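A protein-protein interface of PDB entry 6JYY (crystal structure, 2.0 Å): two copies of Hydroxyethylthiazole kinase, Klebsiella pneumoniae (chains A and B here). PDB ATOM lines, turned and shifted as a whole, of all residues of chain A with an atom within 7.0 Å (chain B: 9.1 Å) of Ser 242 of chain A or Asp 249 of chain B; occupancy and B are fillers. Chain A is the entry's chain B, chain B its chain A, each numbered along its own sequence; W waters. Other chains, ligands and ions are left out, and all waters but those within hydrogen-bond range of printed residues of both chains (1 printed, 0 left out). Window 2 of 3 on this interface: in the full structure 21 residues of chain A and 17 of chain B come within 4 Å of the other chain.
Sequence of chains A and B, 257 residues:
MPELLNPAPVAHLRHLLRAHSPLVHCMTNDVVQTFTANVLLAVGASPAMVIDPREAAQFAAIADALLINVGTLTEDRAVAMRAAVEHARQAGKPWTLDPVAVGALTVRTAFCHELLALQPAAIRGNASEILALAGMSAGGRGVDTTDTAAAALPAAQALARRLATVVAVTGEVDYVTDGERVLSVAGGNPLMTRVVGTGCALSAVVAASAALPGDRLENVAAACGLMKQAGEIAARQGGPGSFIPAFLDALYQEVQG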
ATOM      1  N   LEU A 191       4.020 -28.796 -10.186  1.00  0.00           N
ATOM      2  CA  LEU A 191       4.914 -28.035 -11.068  1.00  0.00           C
ATOM      3  C   LEU A 191       6.358 -28.016 -10.532  1.00  0.00           C
ATOM      4  O   LEU A 191       7.313 -28.001 -11.300  1.00  0.00           O
ATOM      5  CB  LEU A 191       4.402 -26.598 -11.255  1.00  0.00           C
ATOM      6  CG  LEU A 191       5.110 -25.802 -12.363  1.00  0.00           C
ATOM      7  CD1 LEU A 191       4.775 -26.361 -13.760  1.00  0.00           C
ATOM      8  CD2 LEU A 191       4.796 -24.317 -12.307  1.00  0.00           C
ATOM      9  N   ALA A 234       4.700 -19.927  -5.859  1.00  0.00           N
ATOM     10  CA  ALA A 234       5.461 -19.740  -7.079  1.00  0.00           C
ATOM     11  C   ALA A 234       4.785 -20.394  -8.266  1.00  0.00           C
ATOM     12  O   ALA A 234       4.923 -19.929  -9.388  1.00  0.00           O
ATOM     13  CB  ALA A 234       6.864 -20.304  -6.905  1.00  0.00           C
ATOM     14  N   GLN A 237       2.000 -19.262 -11.386  1.00  0.00           N
ATOM     15  CA  GLN A 237       2.401 -18.582 -12.618  1.00  0.00           C
ATOM     16  C   GLN A 237       2.093 -19.493 -13.793  1.00  0.00           C
ATOM     17  O   GLN A 237       1.996 -19.059 -14.939  1.00  0.00           O
ATOM     18  CB  GLN A 237       3.895 -18.241 -12.600  1.00  0.00           C
ATOM     19  CG  GLN A 237       4.261 -17.139 -11.609  1.00  0.00           C
ATOM     20  CD  GLN A 237       4.479 -15.774 -12.259  1.00  0.00           C
ATOM     21  OE1 GLN A 237       5.238 -14.943 -11.739  1.00  0.00           O
ATOM     22  NE2 GLN A 237       3.811 -15.531 -13.393  1.00  0.00           N
ATOM     23  N   GLY A 238       1.954 -20.772 -13.489  1.00  0.00           N
ATOM     24  CA  GLY A 238       1.706 -21.783 -14.491  1.00  0.00           C
ATOM     25  C   GLY A 238       2.991 -22.435 -14.970  1.00  0.00           C
ATOM     26  O   GLY A 238       3.060 -23.663 -15.039  1.00  0.00           O
ATOM     27  N   GLY A 239       4.004 -21.621 -15.280  1.00  0.00           N
ATOM     28  CA  GLY A 239       5.143 -22.095 -16.041  1.00  0.00           C
ATOM     29  C   GLY A 239       6.401 -22.343 -15.231  1.00  0.00           C
ATOM     30  O   GLY A 239       6.694 -21.612 -14.305  1.00  0.00           O
ATOM     31  N   PRO A 240       7.164 -23.375 -15.600  1.00  0.00           N
ATOM     32  CA  PRO A 240       8.369 -23.735 -14.843  1.00  0.00           C
ATOM     33  C   PRO A 240       9.485 -22.677 -14.951  1.00  0.00           C
ATOM     34  O   PRO A 240      10.361 -22.621 -14.097  1.00  0.00           O
ATOM     35  CB  PRO A 240       8.786 -25.061 -15.473  1.00  0.00           C
ATOM     36  CG  PRO A 240       8.301 -24.951 -16.919  1.00  0.00           C
ATOM     37  CD  PRO A 240       7.066 -24.092 -16.890  1.00  0.00           C
ATOM     38  N   GLY A 241       9.423 -21.847 -15.982  1.00  0.00           N
ATOM     39  CA  GLY A 241      10.384 -20.800 -16.190  1.00  0.00           C
ATOM     40  C   GLY A 241      10.193 -19.698 -15.186  1.00  0.00           C
ATOM     41  O   GLY A 241      11.149 -19.237 -14.569  1.00  0.00           O
ATOM     42  N   SER A 242       8.949 -19.282 -14.999  1.00  0.00           N
ATOM     43  CA  SER A 242       8.653 -18.162 -14.117  1.00  0.00           C
ATOM     44  C   SER A 242       8.674 -18.615 -12.664  1.00  0.00           C
ATOM     45  O   SER A 242       8.834 -17.804 -11.757  1.00  0.00           O
ATOM     46  CB  SER A 242       7.296 -17.550 -14.485  1.00  0.00           C
ATOM     47  OG  SER A 242       7.416 -16.688 -15.618  1.00  0.00           O
ATOM     48  N   PHE A 243       8.504 -19.913 -12.455  1.00  0.00           N
ATOM     49  CA  PHE A 243       8.511 -20.500 -11.118  1.00  0.00           C
ATOM     50  C   PHE A 243       9.772 -20.179 -10.308  1.00  0.00           C
ATOM     51  O   PHE A 243       9.700 -19.865  -9.130  1.00  0.00           O
ATOM     52  CB  PHE A 243       8.368 -22.006 -11.226  1.00  0.00           C
ATOM     53  CG  PHE A 243       8.477 -22.724  -9.938  1.00  0.00           C
ATOM     54  CD1 PHE A 243       7.350 -22.944  -9.154  1.00  0.00           C
ATOM     55  CD2 PHE A 243       9.694 -23.224  -9.512  1.00  0.00           C
ATOM     56  CE1 PHE A 243       7.459 -23.648  -7.960  1.00  0.00           C
ATOM     57  CE2 PHE A 243       9.815 -23.909  -8.323  1.00  0.00           C
ATOM     58  CZ  PHE A 243       8.706 -24.125  -7.538  1.00  0.00           C
ATOM     59  N   ILE A 244      10.930 -20.271 -10.942  1.00  0.00           N
ATOM     60  CA  ILE A 244      12.188 -20.188 -10.215  1.00  0.00           C
ATOM     61  C   ILE A 244      12.360 -18.821  -9.542  1.00  0.00           C
ATOM     62  O   ILE A 244      12.534 -18.764  -8.320  1.00  0.00           O
ATOM     63  CB  ILE A 244      13.370 -20.523 -11.159  1.00  0.00           C
ATOM     64  CG1 ILE A 244      13.596 -22.043 -11.181  1.00  0.00           C
ATOM     65  CG2 ILE A 244      14.682 -19.867 -10.710  1.00  0.00           C
ATOM     66  CD1 ILE A 244      13.193 -22.674 -12.481  1.00  0.00           C
ATOM     67  N   PRO A 245      12.274 -17.718 -10.314  1.00  0.00           N
ATOM     68  CA  PRO A 245      12.423 -16.397  -9.684  1.00  0.00           C
ATOM     69  C   PRO A 245      11.313 -16.082  -8.658  1.00  0.00           C
ATOM     70  O   PRO A 245      11.587 -15.470  -7.639  1.00  0.00           O
ATOM     71  CB  PRO A 245      12.371 -15.433 -10.865  1.00  0.00           C
ATOM     72  CG  PRO A 245      11.892 -16.239 -12.032  1.00  0.00           C
ATOM     73  CD  PRO A 245      12.278 -17.630 -11.781  1.00  0.00           C
ATOM     74  N   ALA A 246      10.088 -16.530  -8.926  1.00  0.00           N
ATOM     75  CA  ALA A 246       8.973 -16.364  -7.991  1.00  0.00           C
ATOM     76  C   ALA A 246       9.179 -17.200  -6.704  1.00  0.00           C
ATOM     77  O   ALA A 246       8.803 -16.778  -5.605  1.00  0.00           O
ATOM     78  CB  ALA A 246       7.652 -16.742  -8.682  1.00  0.00           C
ATOM     79  N   PHE A 247       9.772 -18.381  -6.853  1.00  0.00           N
ATOM     80  CA  PHE A 247      10.081 -19.254  -5.736  1.00  0.00           C
ATOM     81  C   PHE A 247      11.088 -18.564  -4.829  1.00  0.00           C
ATOM     82  O   PHE A 247      10.897 -18.497  -3.606  1.00  0.00           O
ATOM     83  CB  PHE A 247      10.622 -20.583  -6.238  1.00  0.00           C
ATOM     84  CG  PHE A 247      10.865 -21.599  -5.175  1.00  0.00           C
ATOM     85  CD1 PHE A 247       9.810 -22.188  -4.501  1.00  0.00           C
ATOM     86  CD2 PHE A 247      12.156 -22.007  -4.866  1.00  0.00           C
ATOM     87  CE1 PHE A 247      10.036 -23.151  -3.537  1.00  0.00           C
ATOM     88  CE2 PHE A 247      12.387 -22.972  -3.898  1.00  0.00           C
ATOM     89  CZ  PHE A 247      11.321 -23.536  -3.224  1.00  0.00           C
ATOM     90  N   ARG B  14       6.146 -31.937 -30.257  1.00  0.00           N
ATOM     91  CA  ARG B  14       5.738 -31.489 -28.921  1.00  0.00           C
ATOM     92  C   ARG B  14       4.928 -32.579 -28.237  1.00  0.00           C
ATOM     93  O   ARG B  14       5.223 -32.974 -27.113  1.00  0.00           O
ATOM     94  CB  ARG B  14       4.892 -30.215 -28.960  1.00  0.00           C
ATOM     95  CG  ARG B  14       5.627 -28.911 -28.801  1.00  0.00           C
ATOM     96  CD  ARG B  14       4.640 -27.796 -28.406  1.00  0.00           C
ATOM     97  NE  ARG B  14       5.330 -26.520 -28.268  1.00  0.00           N
ATOM     98  CZ  ARG B  14       5.310 -25.736 -27.188  1.00  0.00           C
ATOM     99  NH1 ARG B  14       4.593 -26.048 -26.110  1.00  0.00           N
ATOM    100  NH2 ARG B  14       6.003 -24.604 -27.197  1.00  0.00           N
ATOM    101  N   ARG B  18       6.067 -35.325 -24.870  1.00  0.00           N
ATOM    102  CA  ARG B  18       5.239 -35.433 -23.660  1.00  0.00           C
ATOM    103  C   ARG B  18       4.743 -36.821 -23.425  1.00  0.00           C
ATOM    104  O   ARG B  18       4.767 -37.300 -22.289  1.00  0.00           O
ATOM    105  CB  ARG B  18       4.023 -34.522 -23.727  1.00  0.00           C
ATOM    106  CG  ARG B  18       4.263 -33.179 -23.172  1.00  0.00           C
ATOM    107  CD  ARG B  18       3.265 -32.163 -23.683  1.00  0.00           C
ATOM    108  NE  ARG B  18       3.880 -30.842 -23.674  1.00  0.00           N
ATOM    109  CZ  ARG B  18       3.500 -29.820 -24.435  1.00  0.00           C
ATOM    110  NH1 ARG B  18       2.479 -29.938 -25.291  1.00  0.00           N
ATOM    111  NH2 ARG B  18       4.147 -28.669 -24.329  1.00  0.00           N
ATOM    112  N   PHE B  35      20.474 -25.571 -17.236  1.00  0.00           N
ATOM    113  CA  PHE B  35      19.589 -25.139 -18.297  1.00  0.00           C
ATOM    114  C   PHE B  35      19.140 -26.328 -19.171  1.00  0.00           C
ATOM    115  O   PHE B  35      17.971 -26.408 -19.559  1.00  0.00           O
ATOM    116  CB  PHE B  35      20.275 -24.073 -19.144  1.00  0.00           C
ATOM    117  CG  PHE B  35      19.383 -23.454 -20.165  1.00  0.00           C
ATOM    118  CD1 PHE B  35      18.221 -22.808 -19.789  1.00  0.00           C
ATOM    119  CD2 PHE B  35      19.711 -23.498 -21.504  1.00  0.00           C
ATOM    120  CE1 PHE B  35      17.400 -22.237 -20.727  1.00  0.00           C
ATOM    121  CE2 PHE B  35      18.895 -22.905 -22.441  1.00  0.00           C
ATOM    122  CZ  PHE B  35      17.754 -22.268 -22.054  1.00  0.00           C
ATOM    123  N   ASN B  38      16.544 -28.297 -17.175  1.00  0.00           N
ATOM    124  CA  ASN B  38      15.281 -27.570 -17.163  1.00  0.00           C
ATOM    125  C   ASN B  38      14.536 -27.475 -18.529  1.00  0.00           C
ATOM    126  O   ASN B  38      13.304 -27.552 -18.566  1.00  0.00           O
ATOM    127  CB  ASN B  38      15.527 -26.180 -16.582  1.00  0.00           C
ATOM    128  CG  ASN B  38      15.630 -26.202 -15.059  1.00  0.00           C
ATOM    129  OD1 ASN B  38      15.154 -27.141 -14.403  1.00  0.00           O
ATOM    130  ND2 ASN B  38      16.250 -25.189 -14.500  1.00  0.00           N
ATOM    131  N   VAL B  39      15.269 -27.375 -19.637  1.00  0.00           N
ATOM    132  CA  VAL B  39      14.672 -27.487 -20.981  1.00  0.00           C
ATOM    133  C   VAL B  39      14.034 -28.880 -21.204  1.00  0.00           C
ATOM    134  O   VAL B  39      12.897 -28.996 -21.679  1.00  0.00           O
ATOM    135  CB  VAL B  39      15.751 -27.201 -22.074  1.00  0.00           C
ATOM    136  CG1 VAL B  39      15.322 -27.665 -23.459  1.00  0.00           C
ATOM    137  CG2 VAL B  39      16.103 -25.707 -22.084  1.00  0.00           C
ATOM    138  N   ALA B  42      10.959 -29.136 -19.150  1.00  0.00           N
ATOM    139  CA  ALA B  42       9.911 -28.290 -19.694  1.00  0.00           C
ATOM    140  C   ALA B  42       9.192 -28.914 -20.907  1.00  0.00           C
ATOM    141  O   ALA B  42       7.984 -28.652 -21.109  1.00  0.00           O
ATOM    142  CB  ALA B  42      10.455 -26.973 -20.091  1.00  0.00           C
ATOM    143  N   VAL B  43       9.932 -29.639 -21.753  1.00  0.00           N
ATOM    144  CA  VAL B  43       9.282 -30.315 -22.891  1.00  0.00           C
ATOM    145  C   VAL B  43       8.671 -31.655 -22.540  1.00  0.00           C
ATOM    146  O   VAL B  43       8.089 -32.322 -23.416  1.00  0.00           O
ATOM    147  CB  VAL B  43      10.250 -30.545 -24.112  1.00  0.00           C
ATOM    148  CG1 VAL B  43      10.853 -29.209 -24.554  1.00  0.00           C
ATOM    149  CG2 VAL B  43      11.294 -31.597 -23.826  1.00  0.00           C
ATOM    150  N   ALA B 230       9.935 -21.403 -29.670  1.00  0.00           N
ATOM    151  CA  ALA B 230      10.056 -20.971 -28.286  1.00  0.00           C
ATOM    152  C   ALA B 230      10.846 -19.671 -28.187  1.00  0.00           C
ATOM    153  O   ALA B 230      10.469 -18.772 -27.410  1.00  0.00           O
ATOM    154  CB  ALA B 230      10.712 -22.049 -27.447  1.00  0.00           C
ATOM    155  N   ILE B 233       9.042 -16.499 -29.331  1.00  0.00           N
ATOM    156  CA  ILE B 233       8.163 -16.035 -28.237  1.00  0.00           C
ATOM    157  C   ILE B 233       8.930 -15.397 -27.056  1.00  0.00           C
ATOM    158  O   ILE B 233       8.527 -14.370 -26.503  1.00  0.00           O
ATOM    159  CB  ILE B 233       7.308 -17.187 -27.666  1.00  0.00           C
ATOM    160  CG1 ILE B 233       6.266 -17.660 -28.700  1.00  0.00           C
ATOM    161  CG2 ILE B 233       6.583 -16.786 -26.350  1.00  0.00           C
ATOM    162  CD1 ILE B 233       5.686 -19.028 -28.381  1.00  0.00           C
ATOM    163  N   ALA B 234      10.007 -16.026 -26.625  1.00  0.00           N
ATOM    164  CA  ALA B 234      10.719 -15.502 -25.454  1.00  0.00           C
ATOM    165  C   ALA B 234      11.489 -14.209 -25.718  1.00  0.00           C
ATOM    166  O   ALA B 234      11.694 -13.428 -24.789  1.00  0.00           O
ATOM    167  CB  ALA B 234      11.649 -16.549 -24.917  1.00  0.00           C
ATOM    168  N   SER B 242      15.289 -11.820 -19.067  1.00  0.00           N
ATOM    169  CA  SER B 242      13.867 -12.203 -19.073  1.00  0.00           C
ATOM    170  C   SER B 242      13.585 -13.292 -20.104  1.00  0.00           C
ATOM    171  O   SER B 242      12.580 -13.988 -20.013  1.00  0.00           O
ATOM    172  CB  SER B 242      13.005 -10.972 -19.334  1.00  0.00           C
ATOM    173  OG  SER B 242      13.089 -10.096 -18.233  1.00  0.00           O
ATOM    174  N   PHE B 243      14.481 -13.432 -21.078  1.00  0.00           N
ATOM    175  CA  PHE B 243      14.407 -14.509 -22.069  1.00  0.00           C
ATOM    176  C   PHE B 243      14.319 -15.905 -21.442  1.00  0.00           C
ATOM    177  O   PHE B 243      13.506 -16.734 -21.849  1.00  0.00           O
ATOM    178  CB  PHE B 243      15.631 -14.455 -23.012  1.00  0.00           C
ATOM    179  CG  PHE B 243      15.653 -15.559 -24.038  1.00  0.00           C
ATOM    180  CD1 PHE B 243      16.198 -16.802 -23.761  1.00  0.00           C
ATOM    181  CD2 PHE B 243      15.098 -15.352 -25.278  1.00  0.00           C
ATOM    182  CE1 PHE B 243      16.199 -17.818 -24.740  1.00  0.00           C
ATOM    183  CE2 PHE B 243      15.095 -16.360 -26.248  1.00  0.00           C
ATOM    184  CZ  PHE B 243      15.634 -17.583 -25.970  1.00  0.00           C
ATOM    185  N   ILE B 244      15.150 -16.182 -20.443  1.00  0.00           N
ATOM    186  CA  ILE B 244      15.259 -17.545 -19.931  1.00  0.00           C
ATOM    187  C   ILE B 244      13.973 -18.125 -19.270  1.00  0.00           C
ATOM    188  O   ILE B 244      13.488 -19.197 -19.682  1.00  0.00           O
ATOM    189  CB  ILE B 244      16.430 -17.640 -18.945  1.00  0.00           C
ATOM    190  CG1 ILE B 244      17.745 -17.347 -19.689  1.00  0.00           C
ATOM    191  CG2 ILE B 244      16.452 -19.010 -18.309  1.00  0.00           C
ATOM    192  CD1 ILE B 244      18.921 -17.100 -18.813  1.00  0.00           C
ATOM    193  N   PRO B 245      13.412 -17.435 -18.250  1.00  0.00           N
ATOM    194  CA  PRO B 245      12.097 -17.866 -17.749  1.00  0.00           C
ATOM    195  C   PRO B 245      11.007 -17.964 -18.829  1.00  0.00           C
ATOM    196  O   PRO B 245      10.204 -18.904 -18.827  1.00  0.00           O
ATOM    197  CB  PRO B 245      11.723 -16.779 -16.730  1.00  0.00           C
ATOM    198  CG  PRO B 245      12.578 -15.640 -17.041  1.00  0.00           C
ATOM    199  CD  PRO B 245      13.852 -16.184 -17.613  1.00  0.00           C
ATOM    200  N   ALA B 246      10.998 -17.019 -19.759  1.00  0.00           N
ATOM    201  CA  ALA B 246       9.975 -16.992 -20.799  1.00  0.00           C
ATOM    202  C   ALA B 246      10.179 -18.137 -21.810  1.00  0.00           C
ATOM    203  O   ALA B 246       9.230 -18.677 -22.325  1.00  0.00           O
ATOM    204  CB  ALA B 246       9.975 -15.653 -21.500  1.00  0.00           C
ATOM    205  N   PHE B 247      11.427 -18.520 -22.044  1.00  0.00           N
ATOM    206  CA  PHE B 247      11.766 -19.609 -22.956  1.00  0.00           C
ATOM    207  C   PHE B 247      11.261 -20.914 -22.413  1.00  0.00           C
ATOM    208  O   PHE B 247      10.581 -21.716 -23.108  1.00  0.00           O
ATOM    209  CB  PHE B 247      13.275 -19.674 -23.139  1.00  0.00           C
ATOM    210  CG  PHE B 247      13.743 -20.706 -24.146  1.00  0.00           C
ATOM    211  CD1 PHE B 247      13.450 -20.560 -25.501  1.00  0.00           C
ATOM    212  CD2 PHE B 247      14.505 -21.778 -23.748  1.00  0.00           C
ATOM    213  CE1 PHE B 247      13.895 -21.506 -26.441  1.00  0.00           C
ATOM    214  CE2 PHE B 247      14.980 -22.711 -24.679  1.00  0.00           C
ATOM    215  CZ  PHE B 247      14.670 -22.569 -26.027  1.00  0.00           C
ATOM    216  N   LEU B 248      11.616 -21.135 -21.156  1.00  0.00           N
ATOM    217  CA  LEU B 248      11.180 -22.324 -20.471  1.00  0.00           C
ATOM    218  C   LEU B 248       9.662 -22.350 -20.399  1.00  0.00           C
ATOM    219  O   LEU B 248       9.062 -23.392 -20.604  1.00  0.00           O
ATOM    220  CB  LEU B 248      11.784 -22.398 -19.076  1.00  0.00           C
ATOM    221  CG  LEU B 248      13.283 -22.616 -19.109  1.00  0.00           C
ATOM    222  CD1 LEU B 248      13.915 -22.422 -17.700  1.00  0.00           C
ATOM    223  CD2 LEU B 248      13.613 -24.006 -19.667  1.00  0.00           C
ATOM    224  N   ASP B 249       9.046 -21.211 -20.112  1.00  0.00           N
ATOM    225  CA  ASP B 249       7.585 -21.171 -20.066  1.00  0.00           C
ATOM    226  C   ASP B 249       6.977 -21.509 -21.439  1.00  0.00           C
ATOM    227  O   ASP B 249       5.961 -22.190 -21.525  1.00  0.00           O
ATOM    228  CB  ASP B 249       7.060 -19.808 -19.645  1.00  0.00           C
ATOM    229  CG  ASP B 249       7.205 -19.512 -18.136  1.00  0.00           C
ATOM    230  OD1 ASP B 249       7.496 -20.398 -17.299  1.00  0.00           O
ATOM    231  OD2 ASP B 249       6.966 -18.343 -17.808  1.00  0.00           O
ATOM    232  N   ALA B 250       7.585 -20.991 -22.503  1.00  0.00           N
ATOM    233  CA  ALA B 250       7.102 -21.233 -23.857  1.00  0.00           C
ATOM    234  C   ALA B 250       7.194 -22.702 -24.243  1.00  0.00           C
ATOM    235  O   ALA B 250       6.321 -23.214 -24.942  1.00  0.00           O
ATOM    236  CB  ALA B 250       7.875 -20.393 -24.846  1.00  0.00           C
ATOM    237  N   LEU B 251       8.253 -23.380 -23.812  1.00  0.00           N
ATOM    238  CA  LEU B 251       8.359 -24.809 -24.079  1.00  0.00           C
ATOM    239  C   LEU B 251       7.341 -25.711 -23.346  1.00  0.00           C
ATOM    240  O   LEU B 251       7.022 -26.794 -23.814  1.00  0.00           O
ATOM    241  CB  LEU B 251       9.755 -25.289 -23.720  1.00  0.00           C
ATOM    242  CG  LEU B 251      10.896 -24.732 -24.555  1.00  0.00           C
ATOM    243  CD1 LEU B 251      12.219 -25.088 -23.859  1.00  0.00           C
ATOM    244  CD2 LEU B 251      10.859 -25.281 -25.947  1.00  0.00           C
ATOM    245  N   TYR B 252       6.862 -25.286 -22.185  1.00  0.00           N
ATOM    246  CA  TYR B 252       5.982 -26.115 -21.362  1.00  0.00           C
ATOM    247  C   TYR B 252       4.502 -26.067 -21.797  1.00  0.00           C
ATOM    248  O   TYR B 252       3.998 -24.989 -22.082  1.00  0.00           O
ATOM    249  CB  TYR B 252       6.107 -25.658 -19.934  1.00  0.00           C
ATOM    250  CG  TYR B 252       5.247 -26.392 -18.956  1.00  0.00           C
ATOM    251  CD1 TYR B 252       5.560 -27.671 -18.569  1.00  0.00           C
ATOM    252  CD2 TYR B 252       4.146 -25.780 -18.381  1.00  0.00           C
ATOM    253  CE1 TYR B 252       4.805 -28.336 -17.654  1.00  0.00           C
ATOM    254  CE2 TYR B 252       3.382 -26.441 -17.455  1.00  0.00           C
ATOM    255  CZ  TYR B 252       3.716 -27.717 -17.092  1.00  0.00           C
ATOM    256  OH  TYR B 252       2.963 -28.393 -16.166  1.00  0.00           O
HETATM  257  O   HOH W   1       4.304 -17.967 -16.175  1.00  0.00           O
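N of Pro 240 of chain A lies close to OD1 of Asp 249 of chain B (3.4 Å).
The backbone carbonyl oxygen (O) of Gly 239 of chain A lies close to the side-chain carboxylate (OD1) of Asp 249 of chain B (3.3 Å).
The side-chain carboxylate (OD2) of Asp 249 of chain B sits at hydrogen-bond distance from the side-chain hydroxyl (OG) of Ser 242 of chain A (2.8 Å).
The side-chain carboxylate (OD1) of Asp 249 of chain B lies within hydrogen-bond range of the backbone NH (N) of Gly 241 of chain A (2.7 Å).
Hydrophobic or aromatic side chains of chain A within 4 Å of the printed part of chain B: Leu 191 and Pro 240.
Of the 21 printed residues of chain B, 4 touch a printed residue of chain A.
Along chain B the printed residues that touch a printed residue of chain A span positions 245 to 252.
Among the printed residues, 9 pairs touch across the chains.
Among the printed residues, no Asp or Glu carboxylate lies within 4 Å of a Lys or Arg side-chain nitrogen of the other chain.
Positions printed for both chains: 234, 242, 243, 244, 245, 246 and 247.
Of the 9 pairs that touch across the chains among the printed residues, none has its exchanged pair printed and touching as well.
Among the printed residues, pairs that only touch across the chains: Gly 241 of chain A with Pro 245 of chain B (3.3 Å), Pro 240 of chain A with Tyr 252 of chain B (3.6 Å), Gly 241 of chain A with Leu 248 of chain B (3.6 Å), Leu 191 of chain A with Tyr 252 of chain B (3.6 Å) and Gly 238 of chain A with Tyr 252 of chain B (3.7 Å).
Water W1 lies within hydrogen-bond range of the backbone carbonyl oxygen (O) of Gln 237 of chain A, the side-chain carboxylate (OD2) of Asp 249 of chain B and the side-chain hydroxyl (OG) of Ser 242 of chain A.
Of chain A, only Gly 239 (3.0 Å), Pro 240 (3.4 Å), Gly 241 (2.7 Å) and Ser 242 (2.8 Å) come within 4 Å of Asp 249 of chain B.
Printed residues of chain B within 4 Å of Gly 239 of chain A: Asp 249 (3.0 Å).
Of chain B, only Pro 245 (3.3 Å), Leu 248 (3.6 Å) and Asp 249 (2.7 Å) come within 4 Å of Gly 241 of chain A.
Of the printed residues of chain A, Tyr 252 of chain B touches Leu 191 (3.6 Å), Gly 238 (3.7 Å) and Pro 240 (3.6 Å).
Printed residues of chain B within 4 Å of Leu 191 of chain A: Tyr 252.
Of the printed residues of chain B, Gly 238 of chain A touches Tyr 252 (3.7 Å).
The nearest residue of chain A that does not touch Asp 249 of chain B is Phe 243 of chain A (5.0 Å).
The nearest printed residue of chain B that does not touch Gly 238 of chain A is Asp 249 of chain B (5.5 Å).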
